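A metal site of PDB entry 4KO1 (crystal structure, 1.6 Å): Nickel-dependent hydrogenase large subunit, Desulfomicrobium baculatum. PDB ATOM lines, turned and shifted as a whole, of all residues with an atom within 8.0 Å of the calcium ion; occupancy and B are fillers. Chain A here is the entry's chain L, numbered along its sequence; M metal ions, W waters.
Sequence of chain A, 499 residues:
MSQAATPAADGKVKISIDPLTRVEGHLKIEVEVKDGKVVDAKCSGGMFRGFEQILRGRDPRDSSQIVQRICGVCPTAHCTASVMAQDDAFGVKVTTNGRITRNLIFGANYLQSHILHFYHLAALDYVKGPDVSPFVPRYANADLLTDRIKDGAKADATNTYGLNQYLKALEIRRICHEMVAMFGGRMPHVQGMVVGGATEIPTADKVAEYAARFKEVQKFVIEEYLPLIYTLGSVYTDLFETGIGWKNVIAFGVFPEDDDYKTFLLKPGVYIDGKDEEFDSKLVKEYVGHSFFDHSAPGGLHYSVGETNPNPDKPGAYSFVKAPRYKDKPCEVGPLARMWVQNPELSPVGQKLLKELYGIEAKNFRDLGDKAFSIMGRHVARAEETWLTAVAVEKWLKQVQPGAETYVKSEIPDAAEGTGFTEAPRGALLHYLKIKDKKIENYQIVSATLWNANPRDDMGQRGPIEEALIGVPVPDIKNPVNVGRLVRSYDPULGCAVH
OG1 of Thr 308 sits at hydrogen-bond distance from OE2 of Glu 52 (2.6 Å). ND1 of His 499 sits at hydrogen-bond distance from O of Cys 496 (2.8 Å).
Three residues have an atom within 4 Å of the calcium ion: Glu 52, Ile 445 and His 499. The nearest printed residue that does not touch the calcium ion is Glu 286 (4.2 Å).
The calcium ion is bound by water W2 (2.2 Å), water W1 (2.3 Å), water W3 (2.3 Å), O of Ile 445 (2.4 Å), OE1 of Glu 52 (2.4 Å) and NE2 of His 499 (2.5 Å).
Water W1 lies within hydrogen-bond range of OE2 of Glu 286 (2.6 Å), OE1 of Gln 444 (2.8 Å) and NZ of Lys 322 (3.5 Å). Water W2 bridges OE2 of Glu 52 and NZ of Lys 322.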
ATOM      1  N   PHE A  48      34.531   1.639 -32.300  1.00  0.00           N
ATOM      2  CA  PHE A  48      34.588   0.677 -31.208  1.00  0.00           C
ATOM      3  C   PHE A  48      34.998   1.400 -29.932  1.00  0.00           C
ATOM      4  O   PHE A  48      35.906   2.244 -29.963  1.00  0.00           O
ATOM      5  CB  PHE A  48      35.621  -0.404 -31.552  1.00  0.00           C
ATOM      6  CG  PHE A  48      35.940  -1.354 -30.405  1.00  0.00           C
ATOM      7  CD1 PHE A  48      35.080  -2.408 -30.110  1.00  0.00           C
ATOM      8  CD2 PHE A  48      37.094  -1.199 -29.640  1.00  0.00           C
ATOM      9  CE1 PHE A  48      35.368  -3.308 -29.056  1.00  0.00           C
ATOM     10  CE2 PHE A  48      37.393  -2.086 -28.597  1.00  0.00           C
ATOM     11  CZ  PHE A  48      36.516  -3.150 -28.312  1.00  0.00           C
ATOM     12  N   GLU A  52      32.903  -4.054 -22.797  1.00  0.00           N
ATOM     13  CA  GLU A  52      33.126  -5.327 -22.144  1.00  0.00           C
ATOM     14  C   GLU A  52      34.518  -5.373 -21.502  1.00  0.00           C
ATOM     15  O   GLU A  52      34.711  -6.009 -20.461  1.00  0.00           O
ATOM     16  CB  GLU A  52      32.899  -6.490 -23.104  1.00  0.00           C
ATOM     17  CG  GLU A  52      31.444  -6.540 -23.595  1.00  0.00           C
ATOM     18  CD  GLU A  52      31.288  -7.207 -24.949  1.00  0.00           C
ATOM     19  OE1 GLU A  52      30.228  -7.837 -25.182  1.00  0.00           O
ATOM     20  OE2 GLU A  52      32.214  -7.097 -25.794  1.00  0.00           O
ATOM     21  N   GLU A 286      28.316 -16.281 -31.323  1.00  0.00           N
ATOM     22  CA  GLU A 286      28.886 -15.205 -32.124  1.00  0.00           C
ATOM     23  C   GLU A 286      30.114 -15.690 -32.881  1.00  0.00           C
ATOM     24  O   GLU A 286      31.025 -16.290 -32.302  1.00  0.00           O
ATOM     25  CB  GLU A 286      29.241 -14.022 -31.253  1.00  0.00           C
ATOM     26  CG  GLU A 286      28.022 -13.340 -30.634  1.00  0.00           C
ATOM     27  CD  GLU A 286      28.408 -12.170 -29.769  1.00  0.00           C
ATOM     28  OE1 GLU A 286      28.212 -11.019 -30.218  1.00  0.00           O
ATOM     29  OE2 GLU A 286      28.931 -12.399 -28.653  1.00  0.00           O
ATOM     30  N   PHE A 293      38.003  -8.899 -34.458  1.00  0.00           N
ATOM     31  CA  PHE A 293      38.171  -9.546 -33.152  1.00  0.00           C
ATOM     32  C   PHE A 293      38.871 -10.884 -33.277  1.00  0.00           C
ATOM     33  O   PHE A 293      38.723 -11.579 -34.284  1.00  0.00           O
ATOM     34  CB  PHE A 293      36.820  -9.768 -32.468  1.00  0.00           C
ATOM     35  CG  PHE A 293      36.156  -8.486 -32.073  1.00  0.00           C
ATOM     36  CD1 PHE A 293      36.547  -7.800 -30.927  1.00  0.00           C
ATOM     37  CD2 PHE A 293      35.166  -7.935 -32.886  1.00  0.00           C
ATOM     38  CE1 PHE A 293      35.961  -6.581 -30.586  1.00  0.00           C
ATOM     39  CE2 PHE A 293      34.569  -6.725 -32.548  1.00  0.00           C
ATOM     40  CZ  PHE A 293      34.972  -6.043 -31.397  1.00  0.00           C
ATOM     41  N   TYR A 303      27.778 -16.649 -25.648  1.00  0.00           N
ATOM     42  CA  TYR A 303      28.078 -15.401 -24.932  1.00  0.00           C
ATOM     43  C   TYR A 303      28.589 -15.632 -23.511  1.00  0.00           C
ATOM     44  O   TYR A 303      29.331 -14.799 -22.978  1.00  0.00           O
ATOM     45  CB  TYR A 303      26.855 -14.470 -24.917  1.00  0.00           C
ATOM     46  CG  TYR A 303      25.644 -15.103 -24.278  1.00  0.00           C
ATOM     47  CD1 TYR A 303      25.507 -15.140 -22.882  1.00  0.00           C
ATOM     48  CD2 TYR A 303      24.642 -15.683 -25.057  1.00  0.00           C
ATOM     49  CE1 TYR A 303      24.402 -15.737 -22.283  1.00  0.00           C
ATOM     50  CE2 TYR A 303      23.532 -16.282 -24.465  1.00  0.00           C
ATOM     51  CZ  TYR A 303      23.429 -16.312 -23.084  1.00  0.00           C
ATOM     52  OH  TYR A 303      22.323 -16.910 -22.521  1.00  0.00           O
ATOM     53  N   GLY A 306      32.074 -15.564 -23.943  1.00  0.00           N
ATOM     54  CA  GLY A 306      32.423 -14.582 -24.962  1.00  0.00           C
ATOM     55  C   GLY A 306      33.737 -13.891 -24.642  1.00  0.00           C
ATOM     56  O   GLY A 306      34.139 -13.802 -23.483  1.00  0.00           O
ATOM     57  N   GLU A 307      34.400 -13.396 -25.689  1.00  0.00           N
ATOM     58  CA  GLU A 307      35.714 -12.791 -25.576  1.00  0.00           C
ATOM     59  C   GLU A 307      35.717 -11.512 -26.389  1.00  0.00           C
ATOM     60  O   GLU A 307      35.162 -11.478 -27.492  1.00  0.00           O
ATOM     61  CB  GLU A 307      36.778 -13.712 -26.167  1.00  0.00           C
ATOM     62  CG  GLU A 307      37.006 -14.991 -25.375  1.00  0.00           C
ATOM     63  CD  GLU A 307      37.879 -15.984 -26.135  1.00  0.00           C
ATOM     64  OE1 GLU A 307      38.453 -15.606 -27.185  1.00  0.00           O
ATOM     65  OE2 GLU A 307      37.995 -17.144 -25.663  1.00  0.00           O
ATOM     66  N   THR A 308      36.358 -10.491 -25.856  1.00  0.00           N
ATOM     67  CA  THR A 308      36.446  -9.205 -26.530  1.00  0.00           C
ATOM     68  C   THR A 308      37.911  -8.786 -26.635  1.00  0.00           C
ATOM     69  O   THR A 308      38.456  -8.104 -25.745  1.00  0.00           O
ATOM     70  CB  THR A 308      35.571  -8.146 -25.837  1.00  0.00           C
ATOM     71  OG1 THR A 308      34.241  -8.665 -25.743  1.00  0.00           O
ATOM     72  CG2 THR A 308      35.556  -6.840 -26.618  1.00  0.00           C
ATOM     73  N   PHE A 320      33.464  -3.781 -36.941  1.00  0.00           N
ATOM     74  CA  PHE A 320      33.567  -3.975 -35.491  1.00  0.00           C
ATOM     75  C   PHE A 320      32.349  -4.683 -34.891  1.00  0.00           C
ATOM     76  O   PHE A 320      32.296  -4.905 -33.687  1.00  0.00           O
ATOM     77  CB  PHE A 320      33.804  -2.663 -34.758  1.00  0.00           C
ATOM     78  CG  PHE A 320      35.215  -2.150 -34.874  1.00  0.00           C
ATOM     79  CD1 PHE A 320      36.277  -2.815 -34.250  1.00  0.00           C
ATOM     80  CD2 PHE A 320      35.485  -0.980 -35.589  1.00  0.00           C
ATOM     81  CE1 PHE A 320      37.587  -2.337 -34.357  1.00  0.00           C
ATOM     82  CE2 PHE A 320      36.794  -0.488 -35.698  1.00  0.00           C
ATOM     83  CZ  PHE A 320      37.845  -1.172 -35.088  1.00  0.00           C
ATOM     84  N   LYS A 322      30.299  -8.009 -34.282  1.00  0.00           N
ATOM     85  CA  LYS A 322      30.393  -9.484 -34.335  1.00  0.00           C
ATOM     86  C   LYS A 322      29.194 -10.048 -35.097  1.00  0.00           C
ATOM     87  O   LYS A 322      28.263  -9.306 -35.443  1.00  0.00           O
ATOM     88  CB  LYS A 322      30.462 -10.089 -32.927  1.00  0.00           C
ATOM     89  CG  LYS A 322      31.677  -9.642 -32.108  1.00  0.00           C
ATOM     90  CD  LYS A 322      31.784 -10.481 -30.830  1.00  0.00           C
ATOM     91  CE  LYS A 322      32.969 -10.077 -29.963  1.00  0.00           C
ATOM     92  NZ  LYS A 322      32.789 -10.513 -28.516  1.00  0.00           N
ATOM     93  N   LEU A 430      20.525  -9.162 -24.508  1.00  0.00           N
ATOM     94  CA  LEU A 430      20.915  -9.769 -23.239  1.00  0.00           C
ATOM     95  C   LEU A 430      22.232  -9.208 -22.746  1.00  0.00           C
ATOM     96  O   LEU A 430      23.090  -8.799 -23.556  1.00  0.00           O
ATOM     97  CB  LEU A 430      20.948 -11.308 -23.332  1.00  0.00           C
ATOM     98  CG  LEU A 430      22.001 -11.978 -24.213  1.00  0.00           C
ATOM     99  CD1 LEU A 430      23.326 -12.156 -23.447  1.00  0.00           C
ATOM    100  CD2 LEU A 430      21.490 -13.328 -24.742  1.00  0.00           C
ATOM    101  N   TYR A 443      31.858  -9.618 -18.707  1.00  0.00           N
ATOM    102  CA  TYR A 443      30.552  -9.031 -18.984  1.00  0.00           C
ATOM    103  C   TYR A 443      30.402  -9.086 -20.498  1.00  0.00           C
ATOM    104  O   TYR A 443      31.275  -8.605 -21.211  1.00  0.00           O
ATOM    105  CB  TYR A 443      30.516  -7.580 -18.481  1.00  0.00           C
ATOM    106  CG  TYR A 443      29.113  -7.023 -18.278  1.00  0.00           C
ATOM    107  CD1 TYR A 443      28.303  -6.667 -19.367  1.00  0.00           C
ATOM    108  CD2 TYR A 443      28.615  -6.838 -16.990  1.00  0.00           C
ATOM    109  CE1 TYR A 443      27.019  -6.149 -19.154  1.00  0.00           C
ATOM    110  CE2 TYR A 443      27.348  -6.319 -16.778  1.00  0.00           C
ATOM    111  CZ  TYR A 443      26.551  -5.981 -17.858  1.00  0.00           C
ATOM    112  OH  TYR A 443      25.308  -5.448 -17.591  1.00  0.00           O
ATOM    113  N   GLN A 444      29.333  -9.702 -20.971  1.00  0.00           N
ATOM    114  CA  GLN A 444      29.147  -9.859 -22.404  1.00  0.00           C
ATOM    115  C   GLN A 444      27.762  -9.338 -22.795  1.00  0.00           C
ATOM    116  O   GLN A 444      26.765  -9.664 -22.158  1.00  0.00           O
ATOM    117  CB  GLN A 444      29.326 -11.325 -22.831  1.00  0.00           C
ATOM    118  CG  GLN A 444      30.790 -11.801 -22.743  1.00  0.00           C
ATOM    119  CD  GLN A 444      31.680 -11.165 -23.794  1.00  0.00           C
ATOM    120  OE1 GLN A 444      31.364 -11.181 -24.987  1.00  0.00           O
ATOM    121  NE2 GLN A 444      32.811 -10.613 -23.375  1.00  0.00           N
ATOM    122  N   ILE A 445      27.751  -8.497 -23.824  1.00  0.00           N
ATOM    123  CA  ILE A 445      26.533  -7.838 -24.276  1.00  0.00           C
ATOM    124  C   ILE A 445      26.220  -8.375 -25.677  1.00  0.00           C
ATOM    125  O   ILE A 445      27.094  -8.355 -26.547  1.00  0.00           O
ATOM    126  CB  ILE A 445      26.740  -6.319 -24.309  1.00  0.00           C
ATOM    127  CG1 ILE A 445      26.940  -5.812 -22.867  1.00  0.00           C
ATOM    128  CG2 ILE A 445      25.563  -5.610 -24.986  1.00  0.00           C
ATOM    129  CD1 ILE A 445      27.836  -4.662 -22.754  1.00  0.00           C
ATOM    130  N   VAL A 446      24.982  -8.859 -25.866  1.00  0.00           N
ATOM    131  CA  VAL A 446      24.502  -9.284 -27.183  1.00  0.00           C
ATOM    132  C   VAL A 446      23.301  -8.385 -27.432  1.00  0.00           C
ATOM    133  O   VAL A 446      22.230  -8.600 -26.859  1.00  0.00           O
ATOM    134  CB  VAL A 446      24.181 -10.785 -27.198  1.00  0.00           C
ATOM    135  CG1 VAL A 446      23.688 -11.215 -28.568  1.00  0.00           C
ATOM    136  CG2 VAL A 446      25.416 -11.600 -26.768  1.00  0.00           C
ATOM    137  N   SER A 447      23.493  -7.400 -28.307  1.00  0.00           N
ATOM    138  CA  SER A 447      22.525  -6.333 -28.470  1.00  0.00           C
ATOM    139  C   SER A 447      21.676  -6.527 -29.713  1.00  0.00           C
ATOM    140  O   SER A 447      21.918  -7.401 -30.555  1.00  0.00           O
ATOM    141  CB  SER A 447      23.255  -4.997 -28.540  1.00  0.00           C
ATOM    142  OG  SER A 447      24.061  -4.969 -29.695  1.00  0.00           O
ATOM    143  N   LEU A 450      23.209  -5.565 -33.197  1.00  0.00           N
ATOM    144  CA  LEU A 450      24.187  -6.636 -33.401  1.00  0.00           C
ATOM    145  C   LEU A 450      23.595  -7.760 -34.276  1.00  0.00           C
ATOM    146  O   LEU A 450      24.272  -8.283 -35.170  1.00  0.00           O
ATOM    147  CB  LEU A 450      24.645  -7.199 -32.054  1.00  0.00           C
ATOM    148  CG  LEU A 450      25.472  -8.488 -32.096  1.00  0.00           C
ATOM    149  CD1 LEU A 450      26.891  -8.259 -32.640  1.00  0.00           C
ATOM    150  CD2 LEU A 450      25.526  -9.037 -30.692  1.00  0.00           C
ATOM    151  N   CYS A 496      25.132   0.518 -30.051  1.00  0.00           N
ATOM    152  CA  CYS A 496      24.709  -0.749 -29.462  1.00  0.00           C
ATOM    153  C   CYS A 496      25.327  -1.936 -30.144  1.00  0.00           C
ATOM    154  O   CYS A 496      25.684  -2.909 -29.469  1.00  0.00           O
ATOM    155  CB  CYS A 496      23.214  -0.933 -29.540  1.00  0.00           C
ATOM    156  SG  CYS A 496      22.303   0.168 -28.460  1.00  0.00           S
ATOM    157  N   ALA A 497      25.440  -1.873 -31.478  1.00  0.00           N
ATOM    158  CA  ALA A 497      25.906  -3.056 -32.225  1.00  0.00           C
ATOM    159  C   ALA A 497      27.326  -3.436 -31.835  1.00  0.00           C
ATOM    160  O   ALA A 497      27.650  -4.616 -31.783  1.00  0.00           O
ATOM    161  CB  ALA A 497      25.849  -2.823 -33.747  1.00  0.00           C
ATOM    162  N   VAL A 498      28.162  -2.425 -31.562  1.00  0.00           N
ATOM    163  CA  VAL A 498      29.598  -2.630 -31.347  1.00  0.00           C
ATOM    164  C   VAL A 498      29.979  -2.571 -29.868  1.00  0.00           C
ATOM    165  O   VAL A 498      30.775  -3.392 -29.399  1.00  0.00           O
ATOM    166  CB  VAL A 498      30.461  -1.599 -32.126  1.00  0.00           C
ATOM    167  CG1 VAL A 498      31.944  -1.839 -31.821  1.00  0.00           C
ATOM    168  CG2 VAL A 498      30.181  -1.685 -33.635  1.00  0.00           C
ATOM    169  N   HIS A 499      29.418  -1.592 -29.160  1.00  0.00           N
ATOM    170  CA  HIS A 499      29.714  -1.301 -27.757  1.00  0.00           C
ATOM    171  C   HIS A 499      31.215  -1.346 -27.493  1.00  0.00           C
ATOM    172  O   HIS A 499      31.673  -2.003 -26.557  1.00  0.00           O
ATOM    173  CB  HIS A 499      28.879  -2.156 -26.765  1.00  0.00           C
ATOM    174  CG  HIS A 499      28.745  -3.604 -27.154  1.00  0.00           C
ATOM    175  ND1 HIS A 499      27.832  -4.036 -28.090  1.00  0.00           N
ATOM    176  CD2 HIS A 499      29.428  -4.712 -26.764  1.00  0.00           C
ATOM    177  CE1 HIS A 499      27.937  -5.337 -28.251  1.00  0.00           C
ATOM    178  NE2 HIS A 499      28.907  -5.777 -27.452  1.00  0.00           N
ATOM    179  OXT HIS A 499      31.989  -0.729 -28.246  1.00  0.00           O
HETATM  180 CA    CA M   1      29.315  -8.197 -27.332  1.00  0.00          CA
HETATM  181  O   HOH W   1      29.648 -10.477 -27.064  1.00  0.00           O
HETATM  182  O   HOH W   2      31.320  -7.751 -28.211  1.00  0.00           O
HETATM  183  O   HOH W   3      28.743  -8.567 -29.556  1.00  0.00           O
